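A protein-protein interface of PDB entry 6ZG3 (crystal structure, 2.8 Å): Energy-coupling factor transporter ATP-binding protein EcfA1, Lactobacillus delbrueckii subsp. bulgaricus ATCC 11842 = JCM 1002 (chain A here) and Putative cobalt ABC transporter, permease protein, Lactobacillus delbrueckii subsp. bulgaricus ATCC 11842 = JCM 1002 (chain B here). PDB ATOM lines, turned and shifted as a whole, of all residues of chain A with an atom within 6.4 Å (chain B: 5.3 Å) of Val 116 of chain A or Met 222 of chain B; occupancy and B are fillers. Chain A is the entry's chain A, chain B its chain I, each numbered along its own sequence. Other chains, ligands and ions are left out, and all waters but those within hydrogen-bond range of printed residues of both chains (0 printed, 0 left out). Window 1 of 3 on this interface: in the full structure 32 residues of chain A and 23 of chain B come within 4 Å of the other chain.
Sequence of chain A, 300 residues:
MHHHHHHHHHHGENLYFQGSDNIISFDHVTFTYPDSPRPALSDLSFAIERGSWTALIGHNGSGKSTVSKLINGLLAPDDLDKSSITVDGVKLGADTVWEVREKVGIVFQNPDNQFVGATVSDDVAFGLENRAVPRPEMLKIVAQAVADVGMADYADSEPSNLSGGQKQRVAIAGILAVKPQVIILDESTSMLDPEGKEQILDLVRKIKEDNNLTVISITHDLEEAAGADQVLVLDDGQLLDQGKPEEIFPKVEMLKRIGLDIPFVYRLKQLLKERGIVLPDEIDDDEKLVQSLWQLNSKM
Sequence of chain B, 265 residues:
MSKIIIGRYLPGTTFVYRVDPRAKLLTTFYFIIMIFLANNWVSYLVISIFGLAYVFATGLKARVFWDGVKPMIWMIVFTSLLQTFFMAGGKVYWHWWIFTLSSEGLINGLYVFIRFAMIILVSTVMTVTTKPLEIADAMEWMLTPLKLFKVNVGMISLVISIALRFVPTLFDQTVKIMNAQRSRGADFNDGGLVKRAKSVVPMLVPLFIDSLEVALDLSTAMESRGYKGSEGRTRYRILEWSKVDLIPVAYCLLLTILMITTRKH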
ATOM      1  N   TRP A  98       1.761 -10.087  20.870  1.00  0.00           N
ATOM      2  CA  TRP A  98       2.413 -11.224  21.502  1.00  0.00           C
ATOM      3  C   TRP A  98       3.405 -10.757  22.559  1.00  0.00           C
ATOM      4  O   TRP A  98       3.477 -11.344  23.648  1.00  0.00           O
ATOM      5  CB  TRP A  98       3.078 -12.073  20.425  1.00  0.00           C
ATOM      6  CG  TRP A  98       2.124 -12.414  19.312  1.00  0.00           C
ATOM      7  CD1 TRP A  98       1.992 -11.768  18.120  1.00  0.00           C
ATOM      8  CD2 TRP A  98       1.191 -13.490  19.283  1.00  0.00           C
ATOM      9  NE1 TRP A  98       1.026 -12.369  17.352  1.00  0.00           N
ATOM     10  CE2 TRP A  98       0.520 -13.430  18.047  1.00  0.00           C
ATOM     11  CE3 TRP A  98       0.854 -14.497  20.186  1.00  0.00           C
ATOM     12  CZ2 TRP A  98      -0.457 -14.327  17.695  1.00  0.00           C
ATOM     13  CZ3 TRP A  98      -0.117 -15.388  19.832  1.00  0.00           C
ATOM     14  CH2 TRP A  98      -0.761 -15.301  18.595  1.00  0.00           C
ATOM     15  N   ARG A 101       1.361 -10.141  25.451  1.00  0.00           N
ATOM     16  CA  ARG A 101       0.868 -11.344  26.121  1.00  0.00           C
ATOM     17  C   ARG A 101       1.957 -12.027  26.944  1.00  0.00           C
ATOM     18  O   ARG A 101       1.639 -12.763  27.886  1.00  0.00           O
ATOM     19  CB  ARG A 101       0.261 -12.328  25.110  1.00  0.00           C
ATOM     20  CG  ARG A 101      -0.951 -11.752  24.363  1.00  0.00           C
ATOM     21  CD  ARG A 101      -1.631 -12.704  23.371  1.00  0.00           C
ATOM     22  NE  ARG A 101      -2.631 -12.002  22.558  1.00  0.00           N
ATOM     23  CZ  ARG A 101      -3.341 -12.540  21.555  1.00  0.00           C
ATOM     24  NH1 ARG A 101      -3.199 -13.822  21.210  1.00  0.00           N
ATOM     25  NH2 ARG A 101      -4.224 -11.785  20.904  1.00  0.00           N
ATOM     26  N   ASN A 113     -11.084 -26.784  30.169  1.00  0.00           N
ATOM     27  CA  ASN A 113     -11.187 -25.887  29.015  1.00  0.00           C
ATOM     28  C   ASN A 113     -10.081 -24.843  29.034  1.00  0.00           C
ATOM     29  O   ASN A 113     -10.052 -23.958  28.152  1.00  0.00           O
ATOM     30  CB  ASN A 113     -12.521 -25.096  28.901  1.00  0.00           C
ATOM     31  CG  ASN A 113     -13.810 -25.954  29.037  1.00  0.00           C
ATOM     32  OD1 ASN A 113     -13.801 -27.195  29.065  1.00  0.00           O
ATOM     33  ND2 ASN A 113     -14.939 -25.258  29.053  1.00  0.00           N
ATOM     34  N   GLN A 114      -9.186 -24.895  30.016  1.00  0.00           N
ATOM     35  CA  GLN A 114      -7.971 -24.106  30.045  1.00  0.00           C
ATOM     36  C   GLN A 114      -6.786 -25.042  29.972  1.00  0.00           C
ATOM     37  O   GLN A 114      -5.658 -24.597  29.718  1.00  0.00           O
ATOM     38  CB  GLN A 114      -7.907 -23.265  31.334  1.00  0.00           C
ATOM     39  CG  GLN A 114      -7.081 -21.974  31.328  1.00  0.00           C
ATOM     40  CD  GLN A 114      -7.189 -21.231  32.676  1.00  0.00           C
ATOM     41  OE1 GLN A 114      -6.769 -20.075  32.808  1.00  0.00           O
ATOM     42  NE2 GLN A 114      -7.743 -21.914  33.685  1.00  0.00           N
ATOM     43  N   PHE A 115      -7.043 -26.337  30.153  1.00  0.00           N
ATOM     44  CA  PHE A 115      -6.034 -27.388  30.159  1.00  0.00           C
ATOM     45  C   PHE A 115      -5.802 -27.834  28.717  1.00  0.00           C
ATOM     46  O   PHE A 115      -6.694 -28.416  28.091  1.00  0.00           O
ATOM     47  CB  PHE A 115      -6.533 -28.560  31.005  1.00  0.00           C
ATOM     48  CG  PHE A 115      -5.498 -29.182  31.900  1.00  0.00           C
ATOM     49  CD1 PHE A 115      -4.422 -29.869  31.373  1.00  0.00           C
ATOM     50  CD2 PHE A 115      -5.646 -29.138  33.288  1.00  0.00           C
ATOM     51  CE1 PHE A 115      -3.487 -30.477  32.220  1.00  0.00           C
ATOM     52  CE2 PHE A 115      -4.713 -29.744  34.142  1.00  0.00           C
ATOM     53  CZ  PHE A 115      -3.637 -30.405  33.612  1.00  0.00           C
ATOM     54  N   VAL A 116      -4.624 -27.550  28.179  1.00  0.00           N
ATOM     55  CA  VAL A 116      -4.311 -28.089  26.868  1.00  0.00           C
ATOM     56  C   VAL A 116      -3.674 -29.465  26.989  1.00  0.00           C
ATOM     57  O   VAL A 116      -4.038 -30.380  26.245  1.00  0.00           O
ATOM     58  CB  VAL A 116      -3.433 -27.126  26.050  1.00  0.00           C
ATOM     59  CG1 VAL A 116      -4.298 -26.216  25.269  1.00  0.00           C
ATOM     60  CG2 VAL A 116      -2.564 -26.314  26.933  1.00  0.00           C
ATOM     61  N   GLY A 117      -2.761 -29.662  27.943  1.00  0.00           N
ATOM     62  CA  GLY A 117      -1.969 -30.873  27.950  1.00  0.00           C
ATOM     63  C   GLY A 117      -2.708 -32.092  28.476  1.00  0.00           C
ATOM     64  O   GLY A 117      -3.656 -32.011  29.238  1.00  0.00           O
ATOM     65  N   ALA A 118      -2.241 -33.272  28.072  1.00  0.00           N
ATOM     66  CA  ALA A 118      -2.870 -34.491  28.556  1.00  0.00           C
ATOM     67  C   ALA A 118      -2.479 -34.794  29.994  1.00  0.00           C
ATOM     68  O   ALA A 118      -3.119 -35.642  30.642  1.00  0.00           O
ATOM     69  CB  ALA A 118      -2.518 -35.664  27.629  1.00  0.00           C
ATOM     70  N   THR A 119      -1.442 -34.113  30.489  1.00  0.00           N
ATOM     71  CA  THR A 119      -1.025 -34.166  31.877  1.00  0.00           C
ATOM     72  C   THR A 119      -0.594 -32.784  32.339  1.00  0.00           C
ATOM     73  O   THR A 119      -0.310 -31.885  31.537  1.00  0.00           O
ATOM     74  CB  THR A 119       0.123 -35.100  32.090  1.00  0.00           C
ATOM     75  OG1 THR A 119       1.139 -34.755  31.141  1.00  0.00           O
ATOM     76  CG2 THR A 119      -0.330 -36.517  31.917  1.00  0.00           C
ATOM     77  N   ASP A 122       2.727 -31.507  30.858  1.00  0.00           N
ATOM     78  CA  ASP A 122       2.528 -31.088  29.471  1.00  0.00           C
ATOM     79  C   ASP A 122       1.812 -29.729  29.392  1.00  0.00           C
ATOM     80  O   ASP A 122       2.183 -28.834  28.593  1.00  0.00           O
ATOM     81  CB  ASP A 122       1.730 -32.182  28.757  1.00  0.00           C
ATOM     82  CG  ASP A 122       2.587 -33.407  28.393  1.00  0.00           C
ATOM     83  OD1 ASP A 122       3.352 -33.320  27.412  1.00  0.00           O
ATOM     84  OD2 ASP A 122       2.459 -34.465  29.052  1.00  0.00           O
ATOM     85  N   ASP A 123       0.808 -29.549  30.257  1.00  0.00           N
ATOM     86  CA  ASP A 123       0.017 -28.330  30.268  1.00  0.00           C
ATOM     87  C   ASP A 123       0.837 -27.136  30.718  1.00  0.00           C
ATOM     88  O   ASP A 123       0.614 -26.015  30.234  1.00  0.00           O
ATOM     89  CB  ASP A 123      -1.198 -28.491  31.169  1.00  0.00           C
ATOM     90  CG  ASP A 123      -2.147 -27.283  31.107  1.00  0.00           C
ATOM     91  OD1 ASP A 123      -2.849 -27.125  30.079  1.00  0.00           O
ATOM     92  OD2 ASP A 123      -2.212 -26.500  32.095  1.00  0.00           O
ATOM     93  N   PHE A 126       3.362 -26.049  27.827  1.00  0.00           N
ATOM     94  CA  PHE A 126       2.796 -25.446  26.616  1.00  0.00           C
ATOM     95  C   PHE A 126       3.343 -24.034  26.310  1.00  0.00           C
ATOM     96  O   PHE A 126       3.733 -23.748  25.177  1.00  0.00           O
ATOM     97  CB  PHE A 126       1.255 -25.442  26.734  1.00  0.00           C
ATOM     98  CG  PHE A 126       0.535 -24.882  25.506  1.00  0.00           C
ATOM     99  CD1 PHE A 126       0.326 -25.678  24.384  1.00  0.00           C
ATOM    100  CD2 PHE A 126       0.052 -23.582  25.487  1.00  0.00           C
ATOM    101  CE1 PHE A 126      -0.316 -25.185  23.276  1.00  0.00           C
ATOM    102  CE2 PHE A 126      -0.608 -23.091  24.362  1.00  0.00           C
ATOM    103  CZ  PHE A 126      -0.786 -23.902  23.260  1.00  0.00           C
ATOM    104  N   ASN A 130       5.583 -22.658  23.184  1.00  0.00           N
ATOM    105  CA  ASN A 130       5.187 -21.535  22.340  1.00  0.00           C
ATOM    106  C   ASN A 130       6.312 -20.522  22.214  1.00  0.00           C
ATOM    107  O   ASN A 130       6.427 -19.855  21.178  1.00  0.00           O
ATOM    108  CB  ASN A 130       3.931 -20.855  22.902  1.00  0.00           C
ATOM    109  CG  ASN A 130       2.692 -21.727  22.783  1.00  0.00           C
ATOM    110  OD1 ASN A 130       2.779 -22.954  22.750  1.00  0.00           O
ATOM    111  ND2 ASN A 130       1.530 -21.097  22.716  1.00  0.00           N
ATOM    112  N   SER B 161      -3.926 -34.864  20.463  1.00  0.00           N
ATOM    113  CA  SER B 161      -3.612 -34.778  21.889  1.00  0.00           C
ATOM    114  C   SER B 161      -4.758 -34.156  22.671  1.00  0.00           C
ATOM    115  O   SER B 161      -5.210 -34.708  23.685  1.00  0.00           O
ATOM    116  CB  SER B 161      -2.370 -33.922  22.075  1.00  0.00           C
ATOM    117  OG  SER B 161      -1.381 -34.324  21.157  1.00  0.00           O
ATOM    118  N   ILE B 162      -5.229 -32.998  22.207  1.00  0.00           N
ATOM    119  CA  ILE B 162      -6.361 -32.330  22.839  1.00  0.00           C
ATOM    120  C   ILE B 162      -7.577 -33.247  22.859  1.00  0.00           C
ATOM    121  O   ILE B 162      -8.220 -33.435  23.904  1.00  0.00           O
ATOM    122  CB  ILE B 162      -6.645 -30.986  22.138  1.00  0.00           C
ATOM    123  CG1 ILE B 162      -5.450 -30.053  22.347  1.00  0.00           C
ATOM    124  CG2 ILE B 162      -7.908 -30.347  22.667  1.00  0.00           C
ATOM    125  CD1 ILE B 162      -5.382 -28.898  21.419  1.00  0.00           C
ATOM    126  N   ARG B 165      -7.401 -35.876  25.312  1.00  0.00           N
ATOM    127  CA  ARG B 165      -7.410 -35.308  26.650  1.00  0.00           C
ATOM    128  C   ARG B 165      -8.828 -34.988  27.121  1.00  0.00           C
ATOM    129  O   ARG B 165      -9.139 -35.108  28.319  1.00  0.00           O
ATOM    130  CB  ARG B 165      -6.538 -34.047  26.632  1.00  0.00           C
ATOM    131  CG  ARG B 165      -6.559 -33.200  27.894  1.00  0.00           C
ATOM    132  CD  ARG B 165      -7.489 -32.025  27.814  1.00  0.00           C
ATOM    133  NE  ARG B 165      -8.576 -32.267  28.749  1.00  0.00           N
ATOM    134  CZ  ARG B 165      -9.240 -31.309  29.365  1.00  0.00           C
ATOM    135  NH1 ARG B 165      -8.929 -30.036  29.131  1.00  0.00           N
ATOM    136  NH2 ARG B 165     -10.213 -31.623  30.213  1.00  0.00           N
ATOM    137  N   ASP B 217     -13.183 -21.572  24.595  1.00  0.00           N
ATOM    138  CA  ASP B 217     -12.328 -21.293  25.742  1.00  0.00           C
ATOM    139  C   ASP B 217     -10.901 -21.760  25.513  1.00  0.00           C
ATOM    140  O   ASP B 217      -9.946 -21.105  25.955  1.00  0.00           O
ATOM    141  CB  ASP B 217     -12.846 -21.974  27.006  1.00  0.00           C
ATOM    142  CG  ASP B 217     -14.177 -21.465  27.453  1.00  0.00           C
ATOM    143  OD1 ASP B 217     -14.621 -20.406  26.935  1.00  0.00           O
ATOM    144  OD2 ASP B 217     -14.737 -22.118  28.365  1.00  0.00           O
ATOM    145  N   LEU B 218     -10.729 -22.900  24.850  1.00  0.00           N
ATOM    146  CA  LEU B 218      -9.379 -23.382  24.607  1.00  0.00           C
ATOM    147  C   LEU B 218      -8.641 -22.451  23.676  1.00  0.00           C
ATOM    148  O   LEU B 218      -7.506 -22.084  23.953  1.00  0.00           O
ATOM    149  CB  LEU B 218      -9.401 -24.778  24.014  1.00  0.00           C
ATOM    150  CG  LEU B 218      -9.244 -25.956  24.950  1.00  0.00           C
ATOM    151  CD1 LEU B 218      -8.771 -27.160  24.138  1.00  0.00           C
ATOM    152  CD2 LEU B 218      -8.276 -25.595  26.051  1.00  0.00           C
ATOM    153  N   SER B 219      -9.240 -22.095  22.541  1.00  0.00           N
ATOM    154  CA  SER B 219      -8.559 -21.161  21.650  1.00  0.00           C
ATOM    155  C   SER B 219      -8.238 -19.857  22.384  1.00  0.00           C
ATOM    156  O   SER B 219      -7.147 -19.292  22.215  1.00  0.00           O
ATOM    157  CB  SER B 219      -9.366 -20.958  20.346  1.00  0.00           C
ATOM    158  OG  SER B 219     -10.355 -19.932  20.328  1.00  0.00           O
ATOM    159  N   THR B 220      -9.161 -19.386  23.230  1.00  0.00           N
ATOM    160  CA  THR B 220      -8.921 -18.150  23.962  1.00  0.00           C
ATOM    161  C   THR B 220      -7.685 -18.289  24.857  1.00  0.00           C
ATOM    162  O   THR B 220      -6.762 -17.462  24.797  1.00  0.00           O
ATOM    163  CB  THR B 220     -10.191 -17.783  24.758  1.00  0.00           C
ATOM    164  OG1 THR B 220     -10.914 -16.750  24.068  1.00  0.00           O
ATOM    165  CG2 THR B 220      -9.884 -17.356  26.216  1.00  0.00           C
ATOM    166  N   ALA B 221      -7.603 -19.387  25.614  1.00  0.00           N
ATOM    167  CA  ALA B 221      -6.457 -19.611  26.478  1.00  0.00           C
ATOM    168  C   ALA B 221      -5.185 -19.759  25.672  1.00  0.00           C
ATOM    169  O   ALA B 221      -4.184 -19.085  25.935  1.00  0.00           O
ATOM    170  CB  ALA B 221      -6.663 -20.871  27.299  1.00  0.00           C
ATOM    171  N   MET B 222      -5.204 -20.654  24.687  1.00  0.00           N
ATOM    172  CA  MET B 222      -4.024 -20.930  23.879  1.00  0.00           C
ATOM    173  C   MET B 222      -3.420 -19.660  23.303  1.00  0.00           C
ATOM    174  O   MET B 222      -2.199 -19.487  23.318  1.00  0.00           O
ATOM    175  CB  MET B 222      -4.372 -21.883  22.737  1.00  0.00           C
ATOM    176  CG  MET B 222      -4.795 -23.267  23.118  1.00  0.00           C
ATOM    177  SD  MET B 222      -4.811 -24.289  21.621  1.00  0.00           S
ATOM    178  CE  MET B 222      -5.778 -25.602  22.309  1.00  0.00           C
ATOM    179  N   GLU B 223      -4.250 -18.786  22.726  1.00  0.00           N
ATOM    180  CA  GLU B 223      -3.691 -17.543  22.218  1.00  0.00           C
ATOM    181  C   GLU B 223      -3.243 -16.667  23.364  1.00  0.00           C
ATOM    182  O   GLU B 223      -2.326 -15.855  23.210  1.00  0.00           O
ATOM    183  CB  GLU B 223      -4.692 -16.796  21.339  1.00  0.00           C
ATOM    184  CG  GLU B 223      -5.425 -17.665  20.330  1.00  0.00           C
ATOM    185  CD  GLU B 223      -6.459 -16.879  19.559  1.00  0.00           C
ATOM    186  OE1 GLU B 223      -6.121 -15.749  19.127  1.00  0.00           O
ATOM    187  OE2 GLU B 223      -7.610 -17.368  19.406  1.00  0.00           O
ATOM    188  N   SER B 224      -3.877 -16.815  24.519  1.00  0.00           N
ATOM    189  CA  SER B 224      -3.422 -16.041  25.654  1.00  0.00           C
ATOM    190  C   SER B 224      -1.981 -16.385  26.002  1.00  0.00           C
ATOM    191  O   SER B 224      -1.211 -15.487  26.376  1.00  0.00           O
ATOM    192  CB  SER B 224      -4.360 -16.255  26.853  1.00  0.00           C
ATOM    193  OG  SER B 224      -5.711 -15.917  26.546  1.00  0.00           O
ATOM    194  N   ARG B 225      -1.571 -17.650  25.817  1.00  0.00           N
ATOM    195  CA  ARG B 225      -0.225 -18.129  26.158  1.00  0.00           C
ATOM    196  C   ARG B 225       0.737 -18.127  24.961  1.00  0.00           C
ATOM    197  O   ARG B 225       1.707 -18.894  24.940  1.00  0.00           O
ATOM    198  CB  ARG B 225      -0.309 -19.527  26.767  1.00  0.00           C
ATOM    199  CG  ARG B 225      -1.288 -19.603  27.879  1.00  0.00           C
ATOM    200  CD  ARG B 225      -1.526 -20.992  28.260  1.00  0.00           C
ATOM    201  NE  ARG B 225      -0.345 -21.550  28.855  1.00  0.00           N
ATOM    202  CZ  ARG B 225      -0.349 -22.727  29.451  1.00  0.00           C
ATOM    203  NH1 ARG B 225      -1.490 -23.415  29.504  1.00  0.00           N
ATOM    204  NH2 ARG B 225       0.762 -23.198  30.005  1.00  0.00           N
ATOM    205  N   GLY B 226       0.436 -17.343  23.939  1.00  0.00           N
ATOM    206  CA  GLY B 226       1.328 -17.147  22.820  1.00  0.00           C
ATOM    207  C   GLY B 226       1.337 -18.220  21.754  1.00  0.00           C
ATOM    208  O   GLY B 226       2.417 -18.611  21.305  1.00  0.00           O
ATOM    209  N   TYR B 227       0.168 -18.721  21.344  1.00  0.00           N
ATOM    210  CA  TYR B 227       0.102 -19.760  20.314  1.00  0.00           C
ATOM    211  C   TYR B 227       0.009 -19.126  18.921  1.00  0.00           C
ATOM    212  O   TYR B 227      -1.068 -18.791  18.422  1.00  0.00           O
ATOM    213  CB  TYR B 227      -1.053 -20.707  20.579  1.00  0.00           C
ATOM    214  CG  TYR B 227      -1.050 -21.861  19.609  1.00  0.00           C
ATOM    215  CD1 TYR B 227      -1.613 -21.752  18.336  1.00  0.00           C
ATOM    216  CD2 TYR B 227      -0.420 -23.037  19.944  1.00  0.00           C
ATOM    217  CE1 TYR B 227      -1.571 -22.787  17.459  1.00  0.00           C
ATOM    218  CE2 TYR B 227      -0.379 -24.084  19.065  1.00  0.00           C
ATOM    219  CZ  TYR B 227      -0.950 -23.964  17.825  1.00  0.00           C
ATOM    220  OH  TYR B 227      -0.859 -25.061  16.984  1.00  0.00           O
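Trp 98 of chain A touches Gly 226 of chain B (CZ3 to C, 3.7 Å). Tyr 227 of chain B touches Trp 98 of chain A. Ser 224 of chain B touches Arg 101 of chain A (O to CB, 3.7 Å). Asn 113 of chain A touches Leu 218 of chain B (O to CD2, 3.2 Å). O of Phe 115 of chain A touches CD2 of Leu 218 of chain B, 3.8 Å away. Val 116 of chain A touches Met 222 of chain B (CG1 to CE, 3.4 Å). Arg 165 of chain B touches Gly 117 of chain A. Ala 118 of chain A touches Arg 165 of chain B. Arg 225 of chain B touches Phe 126 of chain A. CZ of Phe 126 of chain A touches CD2 of Tyr 227 of chain B, at 3.4 Å.
Gln 114 of chain A touches none of the printed residues of chain B. Of chain B, only Met 222 comes within 4 Å of Val 116 of chain A. Printed residues of chain B within 4 Å of Ala 118 of chain A: Arg 165. Of the printed residues of chain B, Asp 123 of chain A touches Arg 225. Of the printed residues of chain A, Arg 165 of chain B touches Phe 115, Gly 117 and Ala 118. The nearest residue of chain B that does not touch Val 116 of chain A is Arg 225 of chain B (4.02 Å). The nearest residue of chain A that does not touch Met 222 of chain B is Phe 126 of chain A (4.1 Å). The nearest printed residue of chain B that does not touch Phe 126 of chain A is Met 222 of chain B (4.1 Å).
The guanidinium group (NH1) of Arg 101 of chain A is in hydrogen-bond range of the backbone carbonyl oxygen (O) of Glu 223 of chain B. The side-chain carboxylate (OD2) of Asp 217 of chain B lies within hydrogen-bond range of the side-chain amide nitrogen (ND2) of Asn 113 of chain A (3.2 Å). O of Phe 115 of chain A is in hydrogen-bond range of NH1 of Arg 165 of chain B, at 2.9 Å. The side-chain carboxylate (OD1) of Asp 123 of chain A is in salt-bridge range of the guanidinium group (NH1) of Arg 225 of chain B (3.99 Å). The side-chain amide nitrogen (ND2) of Asn 130 of chain A lies within hydrogen-bond range of the backbone carbonyl oxygen (O) of Arg 225 of chain B (3.1 Å). ND2 of Asn 130 of chain A lies within hydrogen-bond range of O of Gly 226 of chain B, at 3.0 Å. ND2 of Asn 130 of chain A lies close to N of Tyr 227 of chain B (3.1 Å).
Of the 14 printed residues of chain B, 9 touch a printed residue of chain A. Hydrophobic or aromatic side chains of chain A within 4 Å of the printed part of chain B: Trp 98, Phe 115, Val 116 and Phe 126.
N of Val 116 of chain A is in hydrogen-bond range of OD1 of Asp 123 of chain A, 2.6 Å away. The backbone NH (N) of Gly 117 of chain A is in hydrogen-bond range of the side-chain carboxylate (OD1) of Asp 123 of chain A (3.3 Å). OD1 of Asn 130 of chain A sits close to O of Phe 126 of chain A, 2.7 Å away. O of Thr 220 of chain B lies within hydrogen-bond range of OG of Ser 224 of chain B (2.6 Å). The backbone NH of Tyr 227 of chain B sits at hydrogen-bond distance from the backbone carbonyl oxygen of Met 222 of chain B, at 3.2 Å.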
